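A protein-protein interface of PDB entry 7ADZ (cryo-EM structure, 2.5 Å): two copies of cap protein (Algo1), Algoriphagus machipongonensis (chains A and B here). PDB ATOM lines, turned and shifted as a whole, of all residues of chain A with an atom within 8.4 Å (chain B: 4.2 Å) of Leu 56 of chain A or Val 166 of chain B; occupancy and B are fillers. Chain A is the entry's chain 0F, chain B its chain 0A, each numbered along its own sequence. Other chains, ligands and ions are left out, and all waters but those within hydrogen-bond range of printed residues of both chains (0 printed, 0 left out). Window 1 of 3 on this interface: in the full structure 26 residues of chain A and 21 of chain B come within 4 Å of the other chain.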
ATOM      1  N   ILE A   2      -9.786   0.424  -8.617  1.00  0.00           N
ATOM      2  CA  ILE A   2      -8.604   0.665  -7.794  1.00  0.00           C
ATOM      3  C   ILE A   2      -7.406   1.027  -8.664  1.00  0.00           C
ATOM      4  O   ILE A   2      -6.659   1.963  -8.359  1.00  0.00           O
ATOM      5  CB  ILE A   2      -8.310  -0.551  -6.897  1.00  0.00           C
ATOM      6  CG1 ILE A   2      -9.529  -0.881  -6.036  1.00  0.00           C
ATOM      7  CG2 ILE A   2      -7.110  -0.285  -6.003  1.00  0.00           C
ATOM      8  CD1 ILE A   2      -9.371  -2.131  -5.206  1.00  0.00           C
ATOM      9  N   LEU A   6      -5.488   5.035  -9.158  1.00  0.00           N
ATOM     10  CA  LEU A   6      -4.074   5.184  -8.826  1.00  0.00           C
ATOM     11  C   LEU A   6      -3.241   5.510 -10.060  1.00  0.00           C
ATOM     12  O   LEU A   6      -2.189   6.149  -9.953  1.00  0.00           O
ATOM     13  CB  LEU A   6      -3.560   3.918  -8.142  1.00  0.00           C
ATOM     14  CG  LEU A   6      -4.144   3.611  -6.757  1.00  0.00           C
ATOM     15  CD1 LEU A   6      -3.375   2.506  -6.077  1.00  0.00           C
ATOM     16  CD2 LEU A   6      -4.176   4.849  -5.874  1.00  0.00           C
ATOM     17  N   MET A  53       0.021   0.740  -2.329  1.00  0.00           N
ATOM     18  CA  MET A  53      -1.170   0.653  -1.484  1.00  0.00           C
ATOM     19  C   MET A  53      -0.875  -0.286  -0.318  1.00  0.00           C
ATOM     20  O   MET A  53      -0.436  -1.419  -0.528  1.00  0.00           O
ATOM     21  CB  MET A  53      -2.373   0.165  -2.285  1.00  0.00           C
ATOM     22  CG  MET A  53      -3.660   0.092  -1.480  1.00  0.00           C
ATOM     23  SD  MET A  53      -4.905  -0.991  -2.206  1.00  0.00           S
ATOM     24  CE  MET A  53      -4.064  -2.569  -2.142  1.00  0.00           C
ATOM     25  N   ILE A  54      -1.111   0.180   0.910  1.00  0.00           N
ATOM     26  CA  ILE A  54      -0.710  -0.619   2.064  1.00  0.00           C
ATOM     27  C   ILE A  54      -1.914  -1.130   2.859  1.00  0.00           C
ATOM     28  O   ILE A  54      -1.793  -2.109   3.602  1.00  0.00           O
ATOM     29  CB  ILE A  54       0.281   0.166   2.950  1.00  0.00           C
ATOM     30  CG1 ILE A  54      -0.361   1.408   3.564  1.00  0.00           C
ATOM     31  CG2 ILE A  54       1.525   0.536   2.157  1.00  0.00           C
ATOM     32  CD1 ILE A  54       0.591   2.289   4.330  1.00  0.00           C
ATOM     33  N   ASN A  55      -3.091  -0.513   2.728  1.00  0.00           N
ATOM     34  CA  ASN A  55      -4.245  -0.953   3.509  1.00  0.00           C
ATOM     35  C   ASN A  55      -5.553  -0.579   2.813  1.00  0.00           C
ATOM     36  O   ASN A  55      -5.597   0.304   1.959  1.00  0.00           O
ATOM     37  CB  ASN A  55      -4.201  -0.364   4.924  1.00  0.00           C
ATOM     38  CG  ASN A  55      -4.927  -1.219   5.933  1.00  0.00           C
ATOM     39  OD1 ASN A  55      -5.370  -2.322   5.622  1.00  0.00           O
ATOM     40  ND2 ASN A  55      -5.045  -0.720   7.153  1.00  0.00           N
ATOM     41  N   LEU A  56      -6.632  -1.265   3.210  1.00  0.00           N
ATOM     42  CA  LEU A  56      -7.995  -1.005   2.755  1.00  0.00           C
ATOM     43  C   LEU A  56      -8.951  -0.965   3.938  1.00  0.00           C
ATOM     44  O   LEU A  56      -8.894  -1.817   4.823  1.00  0.00           O
ATOM     45  CB  LEU A  56      -8.519  -2.086   1.800  1.00  0.00           C
ATOM     46  CG  LEU A  56      -7.929  -2.314   0.420  1.00  0.00           C
ATOM     47  CD1 LEU A  56      -8.592  -3.500  -0.222  1.00  0.00           C
ATOM     48  CD2 LEU A  56      -8.159  -1.108  -0.402  1.00  0.00           C
ATOM     49  N   ARG A  57      -9.861   0.008   3.928  1.00  0.00           N
ATOM     50  CA  ARG A  57     -10.920   0.096   4.928  1.00  0.00           C
ATOM     51  C   ARG A  57     -12.252   0.320   4.222  1.00  0.00           C
ATOM     52  O   ARG A  57     -12.312   0.523   3.010  1.00  0.00           O
ATOM     53  CB  ARG A  57     -10.676   1.222   5.946  1.00  0.00           C
ATOM     54  CG  ARG A  57      -9.253   1.352   6.472  1.00  0.00           C
ATOM     55  CD  ARG A  57      -8.887   0.252   7.453  1.00  0.00           C
ATOM     56  NE  ARG A  57      -9.230   0.628   8.820  1.00  0.00           N
ATOM     57  CZ  ARG A  57      -9.994  -0.099   9.625  1.00  0.00           C
ATOM     58  NH1 ARG A  57     -10.259   0.327  10.850  1.00  0.00           N
ATOM     59  NH2 ARG A  57     -10.479  -1.258   9.214  1.00  0.00           N
ATOM     60  N   GLU A  58     -13.331   0.287   4.999  1.00  0.00           N
ATOM     61  CA  GLU A  58     -14.685   0.472   4.490  1.00  0.00           C
ATOM     62  C   GLU A  58     -15.344   1.642   5.210  1.00  0.00           C
ATOM     63  O   GLU A  58     -15.250   1.753   6.435  1.00  0.00           O
ATOM     64  CB  GLU A  58     -15.518  -0.797   4.671  1.00  0.00           C
ATOM     65  CG  GLU A  58     -16.907  -0.717   4.068  1.00  0.00           C
ATOM     66  CD  GLU A  58     -17.711  -1.976   4.294  1.00  0.00           C
ATOM     67  OE1 GLU A  58     -17.191  -2.894   4.961  1.00  0.00           O
ATOM     68  OE2 GLU A  58     -18.860  -2.049   3.811  1.00  0.00           O
ATOM     69  N   GLU A  59     -15.997   2.516   4.447  1.00  0.00           N
ATOM     70  CA  GLU A  59     -16.722   3.635   5.034  1.00  0.00           C
ATOM     71  C   GLU A  59     -18.028   3.167   5.666  1.00  0.00           C
ATOM     72  O   GLU A  59     -18.879   2.573   5.000  1.00  0.00           O
ATOM     73  CB  GLU A  59     -16.992   4.702   3.972  1.00  0.00           C
ATOM     74  CG  GLU A  59     -17.821   5.878   4.472  1.00  0.00           C
ATOM     75  CD  GLU A  59     -17.120   6.697   5.539  1.00  0.00           C
ATOM     76  OE1 GLU A  59     -15.877   6.817   5.495  1.00  0.00           O
ATOM     77  OE2 GLU A  59     -17.814   7.204   6.443  1.00  0.00           O
ATOM     78  N   ASN A  83     -18.276   1.231  -0.495  1.00  0.00           N
ATOM     79  CA  ASN A  83     -17.391   2.397  -0.492  1.00  0.00           C
ATOM     80  C   ASN A  83     -16.111   2.107   0.293  1.00  0.00           C
ATOM     81  O   ASN A  83     -16.168   1.591   1.411  1.00  0.00           O
ATOM     82  CB  ASN A  83     -18.116   3.614   0.086  1.00  0.00           C
ATOM     83  CG  ASN A  83     -19.484   3.839  -0.540  1.00  0.00           C
ATOM     84  OD1 ASN A  83     -19.600   4.432  -1.607  1.00  0.00           O
ATOM     85  ND2 ASN A  83     -20.528   3.378   0.132  1.00  0.00           N
ATOM     86  N   ILE A  84     -14.961   2.461  -0.289  1.00  0.00           N
ATOM     87  CA  ILE A  84     -13.641   2.020   0.171  1.00  0.00           C
ATOM     88  C   ILE A  84     -12.718   3.227   0.350  1.00  0.00           C
ATOM     89  O   ILE A  84     -12.630   4.082  -0.537  1.00  0.00           O
ATOM     90  CB  ILE A  84     -13.025   1.008  -0.821  1.00  0.00           C
ATOM     91  CG1 ILE A  84     -13.857  -0.270  -0.902  1.00  0.00           C
ATOM     92  CG2 ILE A  84     -11.614   0.618  -0.438  1.00  0.00           C
ATOM     93  CD1 ILE A  84     -14.035  -0.957   0.419  1.00  0.00           C
ATOM     94  N   ASN A  85     -12.021   3.285   1.490  1.00  0.00           N
ATOM     95  CA  ASN A  85     -10.901   4.199   1.717  1.00  0.00           C
ATOM     96  C   ASN A  85      -9.575   3.474   1.512  1.00  0.00           C
ATOM     97  O   ASN A  85      -9.475   2.273   1.772  1.00  0.00           O
ATOM     98  CB  ASN A  85     -10.940   4.773   3.135  1.00  0.00           C
ATOM     99  CG  ASN A  85     -12.043   5.786   3.332  1.00  0.00           C
ATOM    100  OD1 ASN A  85     -12.292   6.627   2.474  1.00  0.00           O
ATOM    101  ND2 ASN A  85     -12.711   5.716   4.471  1.00  0.00           N
ATOM    102  N   LEU A  86      -8.546   4.206   1.072  1.00  0.00           N
ATOM    103  CA  LEU A  86      -7.214   3.644   0.855  1.00  0.00           C
ATOM    104  C   LEU A  86      -6.184   4.308   1.762  1.00  0.00           C
ATOM    105  O   LEU A  86      -6.377   5.434   2.224  1.00  0.00           O
ATOM    106  CB  LEU A  86      -6.730   3.816  -0.591  1.00  0.00           C
ATOM    107  CG  LEU A  86      -7.539   3.520  -1.852  1.00  0.00           C
ATOM    108  CD1 LEU A  86      -6.612   3.458  -3.051  1.00  0.00           C
ATOM    109  CD2 LEU A  86      -8.339   2.266  -1.752  1.00  0.00           C
ATOM    110  N   PHE A  87      -5.077   3.605   1.999  1.00  0.00           N
ATOM    111  CA  PHE A  87      -3.898   4.162   2.657  1.00  0.00           C
ATOM    112  C   PHE A  87      -2.682   3.944   1.765  1.00  0.00           C
ATOM    113  O   PHE A  87      -2.385   2.810   1.384  1.00  0.00           O
ATOM    114  CB  PHE A  87      -3.681   3.533   4.031  1.00  0.00           C
ATOM    115  CG  PHE A  87      -4.492   4.166   5.119  1.00  0.00           C
ATOM    116  CD1 PHE A  87      -4.066   5.334   5.723  1.00  0.00           C
ATOM    117  CD2 PHE A  87      -5.676   3.589   5.548  1.00  0.00           C
ATOM    118  CE1 PHE A  87      -4.808   5.920   6.730  1.00  0.00           C
ATOM    119  CE2 PHE A  87      -6.426   4.172   6.551  1.00  0.00           C
ATOM    120  CZ  PHE A  87      -5.990   5.336   7.144  1.00  0.00           C
ATOM    121  N   LEU A  88      -1.979   5.029   1.441  1.00  0.00           N
ATOM    122  CA  LEU A  88      -0.932   5.020   0.433  1.00  0.00           C
ATOM    123  C   LEU A  88       0.401   5.489   1.006  1.00  0.00           C
ATOM    124  O   LEU A  88       0.459   6.141   2.050  1.00  0.00           O
ATOM    125  CB  LEU A  88      -1.309   5.908  -0.756  1.00  0.00           C
ATOM    126  CG  LEU A  88      -2.649   5.599  -1.414  1.00  0.00           C
ATOM    127  CD1 LEU A  88      -2.986   6.651  -2.454  1.00  0.00           C
ATOM    128  CD2 LEU A  88      -2.632   4.213  -2.026  1.00  0.00           C
ATOM    129  N   ILE A 173     -13.428   5.543  -3.048  1.00  0.00           N
ATOM    130  CA  ILE A 173     -13.591   4.805  -4.297  1.00  0.00           C
ATOM    131  C   ILE A 173     -14.905   4.032  -4.219  1.00  0.00           C
ATOM    132  O   ILE A 173     -15.154   3.323  -3.239  1.00  0.00           O
ATOM    133  CB  ILE A 173     -12.408   3.855  -4.546  1.00  0.00           C
ATOM    134  CG1 ILE A 173     -11.109   4.651  -4.610  1.00  0.00           C
ATOM    135  CG2 ILE A 173     -12.616   3.060  -5.819  1.00  0.00           C
ATOM    136  CD1 ILE A 173      -9.891   3.813  -4.856  1.00  0.00           C
ATOM    137  N   ILE A 175     -17.390   1.153  -5.542  1.00  0.00           N
ATOM    138  CA  ILE A 175     -17.381  -0.150  -6.206  1.00  0.00           C
ATOM    139  C   ILE A 175     -18.814  -0.669  -6.255  1.00  0.00           C
ATOM    140  O   ILE A 175     -19.461  -0.818  -5.212  1.00  0.00           O
ATOM    141  CB  ILE A 175     -16.456  -1.141  -5.484  1.00  0.00           C
ATOM    142  CG1 ILE A 175     -14.997  -0.734  -5.678  1.00  0.00           C
ATOM    143  CG2 ILE A 175     -16.688  -2.563  -5.974  1.00  0.00           C
ATOM    144  CD1 ILE A 175     -14.023  -1.640  -4.993  1.00  0.00           C
ATOM    145  N   ILE B  89      -8.042 -15.513   2.836  1.00  0.00           N
ATOM    146  CA  ILE B  89      -7.318 -14.447   2.154  1.00  0.00           C
ATOM    147  C   ILE B  89      -7.328 -14.726   0.653  1.00  0.00           C
ATOM    148  O   ILE B  89      -7.258 -15.881   0.221  1.00  0.00           O
ATOM    149  CB  ILE B  89      -5.872 -14.291   2.708  1.00  0.00           C
ATOM    150  CG1 ILE B  89      -5.184 -13.037   2.146  1.00  0.00           C
ATOM    151  CG2 ILE B  89      -5.019 -15.542   2.488  1.00  0.00           C
ATOM    152  CD1 ILE B  89      -3.780 -12.820   2.634  1.00  0.00           C
ATOM    153  N   PHE B  90      -7.483 -13.670  -0.141  1.00  0.00           N
ATOM    154  CA  PHE B  90      -7.201 -13.699  -1.569  1.00  0.00           C
ATOM    155  C   PHE B  90      -5.948 -12.869  -1.800  1.00  0.00           C
ATOM    156  O   PHE B  90      -5.961 -11.657  -1.576  1.00  0.00           O
ATOM    157  CB  PHE B  90      -8.364 -13.140  -2.389  1.00  0.00           C
ATOM    158  CG  PHE B  90      -9.545 -14.059  -2.496  1.00  0.00           C
ATOM    159  CD1 PHE B  90      -9.633 -14.975  -3.527  1.00  0.00           C
ATOM    160  CD2 PHE B  90     -10.584 -13.985  -1.584  1.00  0.00           C
ATOM    161  CE1 PHE B  90     -10.725 -15.815  -3.639  1.00  0.00           C
ATOM    162  CE2 PHE B  90     -11.682 -14.819  -1.693  1.00  0.00           C
ATOM    163  CZ  PHE B  90     -11.751 -15.735  -2.721  1.00  0.00           C
ATOM    164  N   LEU B 104      -8.044  -7.605  -8.049  1.00  0.00           N
ATOM    165  CA  LEU B 104      -8.623  -7.391  -6.727  1.00  0.00           C
ATOM    166  C   LEU B 104      -9.936  -6.624  -6.809  1.00  0.00           C
ATOM    167  O   LEU B 104     -10.813  -6.797  -5.957  1.00  0.00           O
ATOM    168  CB  LEU B 104      -7.633  -6.660  -5.827  1.00  0.00           C
ATOM    169  CG  LEU B 104      -6.543  -7.504  -5.168  1.00  0.00           C
ATOM    170  CD1 LEU B 104      -5.824  -6.678  -4.119  1.00  0.00           C
ATOM    171  CD2 LEU B 104      -7.107  -8.783  -4.561  1.00  0.00           C
ATOM    172  N   LEU B 108     -13.648  -8.040  -5.435  1.00  0.00           N
ATOM    173  CA  LEU B 108     -14.506  -7.186  -4.616  1.00  0.00           C
ATOM    174  C   LEU B 108     -15.856  -6.937  -5.282  1.00  0.00           C
ATOM    175  O   LEU B 108     -16.874  -6.791  -4.597  1.00  0.00           O
ATOM    176  CB  LEU B 108     -13.806  -5.857  -4.334  1.00  0.00           C
ATOM    177  CG  LEU B 108     -12.705  -5.836  -3.273  1.00  0.00           C
ATOM    178  CD1 LEU B 108     -11.953  -4.526  -3.326  1.00  0.00           C
ATOM    179  CD2 LEU B 108     -13.287  -6.061  -1.893  1.00  0.00           C
ATOM    180  N   THR B 145     -11.971  -6.168   7.136  1.00  0.00           N
ATOM    181  CA  THR B 145     -10.872  -5.221   6.963  1.00  0.00           C
ATOM    182  C   THR B 145     -10.158  -5.002   8.292  1.00  0.00           C
ATOM    183  O   THR B 145     -10.764  -4.456   9.229  1.00  0.00           O
ATOM    184  CB  THR B 145     -11.369  -3.882   6.399  1.00  0.00           C
ATOM    185  OG1 THR B 145     -12.373  -3.328   7.259  1.00  0.00           O
ATOM    186  CG2 THR B 145     -11.948  -4.065   5.003  1.00  0.00           C
ATOM    187  N   SER B 165      -3.952  -7.705  -1.187  1.00  0.00           N
ATOM    188  CA  SER B 165      -4.738  -8.772  -0.584  1.00  0.00           C
ATOM    189  C   SER B 165      -6.076  -8.230  -0.100  1.00  0.00           C
ATOM    190  O   SER B 165      -6.210  -7.051   0.225  1.00  0.00           O
ATOM    191  CB  SER B 165      -3.972  -9.406   0.578  1.00  0.00           C
ATOM    192  OG  SER B 165      -2.962 -10.272   0.109  1.00  0.00           O
ATOM    193  N   VAL B 166      -7.064  -9.124  -0.042  1.00  0.00           N
ATOM    194  CA  VAL B 166      -8.343  -8.871   0.612  1.00  0.00           C
ATOM    195  C   VAL B 166      -8.649 -10.045   1.529  1.00  0.00           C
ATOM    196  O   VAL B 166      -8.204 -11.171   1.296  1.00  0.00           O
ATOM    197  CB  VAL B 166      -9.506  -8.644  -0.386  1.00  0.00           C
ATOM    198  CG1 VAL B 166      -9.420  -7.259  -0.997  1.00  0.00           C
ATOM    199  CG2 VAL B 166      -9.514  -9.705  -1.471  1.00  0.00           C
ATOM    200  N   PHE B 167      -9.418  -9.777   2.576  1.00  0.00           N
ATOM    201  CA  PHE B 167      -9.714 -10.759   3.610  1.00  0.00           C
ATOM    202  C   PHE B 167     -11.216 -10.991   3.705  1.00  0.00           C
ATOM    203  O   PHE B 167     -12.003 -10.049   3.616  1.00  0.00           O
ATOM    204  CB  PHE B 167      -9.162 -10.301   4.962  1.00  0.00           C
ATOM    205  CG  PHE B 167      -7.662 -10.219   5.009  1.00  0.00           C
ATOM    206  CD1 PHE B 167      -6.911 -11.323   5.370  1.00  0.00           C
ATOM    207  CD2 PHE B 167      -7.002  -9.040   4.691  1.00  0.00           C
ATOM    208  CE1 PHE B 167      -5.536 -11.257   5.419  1.00  0.00           C
ATOM    209  CE2 PHE B 167      -5.626  -8.970   4.731  1.00  0.00           C
ATOM    210  CZ  PHE B 167      -4.891 -10.080   5.099  1.00  0.00           C
ATOM    211  N   TYR B 168     -11.611 -12.249   3.888  1.00  0.00           N
ATOM    212  CA  TYR B 168     -13.019 -12.610   3.976  1.00  0.00           C
ATOM    213  C   TYR B 168     -13.263 -13.563   5.134  1.00  0.00           C
ATOM    214  O   TYR B 168     -12.361 -14.272   5.581  1.00  0.00           O
ATOM    215  CB  TYR B 168     -13.519 -13.250   2.678  1.00  0.00           C
ATOM    216  CG  TYR B 168     -13.834 -12.246   1.602  1.00  0.00           C
ATOM    217  CD1 TYR B 168     -15.066 -11.613   1.564  1.00  0.00           C
ATOM    218  CD2 TYR B 168     -12.890 -11.914   0.637  1.00  0.00           C
ATOM    219  CE1 TYR B 168     -15.357 -10.687   0.586  1.00  0.00           C
ATOM    220  CE2 TYR B 168     -13.170 -10.994  -0.340  1.00  0.00           C
ATOM    221  CZ  TYR B 168     -14.406 -10.386  -0.364  1.00  0.00           C
ATOM    222  OH  TYR B 168     -14.688  -9.466  -1.339  1.00  0.00           O
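NH2 of Arg 57 of chain A lies within hydrogen-bond range of O of Thr 145 of chain B, at 3.2 Å.
Of the printed residues of chain B, Ile 2 of chain A touches Leu 108.
Of chain B, only Thr 145 (3.6 Å) and Val 166 (3.9 Å) come within 4 Å of Leu 56 of chain A.
Of the printed residues of chain B, Arg 57 of chain A touches Thr 145.
Printed residues of chain B within 4 Å of Ile 175 of chain A: Leu 108 (3.9 Å).
Of the printed residues of chain A, Leu 108 of chain B touches Ile 2 and Ile 175.
Printed residues of chain A within 4 Å of Thr 145 of chain B: Leu 56 and Arg 57.
No residue of chain A comes within 4 Å of Ser 165 of chain B.
Of chain A, only Leu 56 comes within 4 Å of Val 166 of chain B.
The nearest printed residue of chain B that does not touch Arg 57 of chain A is Leu 108 of chain B (8.1 Å).
Among the printed residues, merely in contact across the chains: Leu 56 of chain A with Thr 145 of chain B, Ile 175 of chain A with Leu 108 of chain B, Leu 56 of chain A with Val 166 of chain B and Ile 2 of chain A with Leu 108 of chain B.
Of the 17 printed residues of chain A, 4 touch a printed residue of chain B.
Hydrophobic or aromatic side chains of chain A that line the printed part of chain B: Ile 2, Leu 56 and Ile 175.
Of the 9 printed residues of chain B, 3 touch a printed residue of chain A.
Printed residues of chain B that touch a printed residue of chain A: Leu 108, Thr 145 and Val 166.
Hydrophobic or aromatic side chains of chain B within 4 Å of the printed part of chain A: Leu 108 and Val 166.
Among the printed residues, 5 pairs touch across the chains.
Among the printed residues, no Asp or Glu carboxylate lies within 4 Å of a Lys or Arg side-chain nitrogen of the other chain.
O of Asn 85 of chain A sits at hydrogen-bond distance from N of Arg 57 of chain A.
N of Phe 90 of chain B is in hydrogen-bond range of O of Val 166 of chain B.
No position is printed for both chains.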
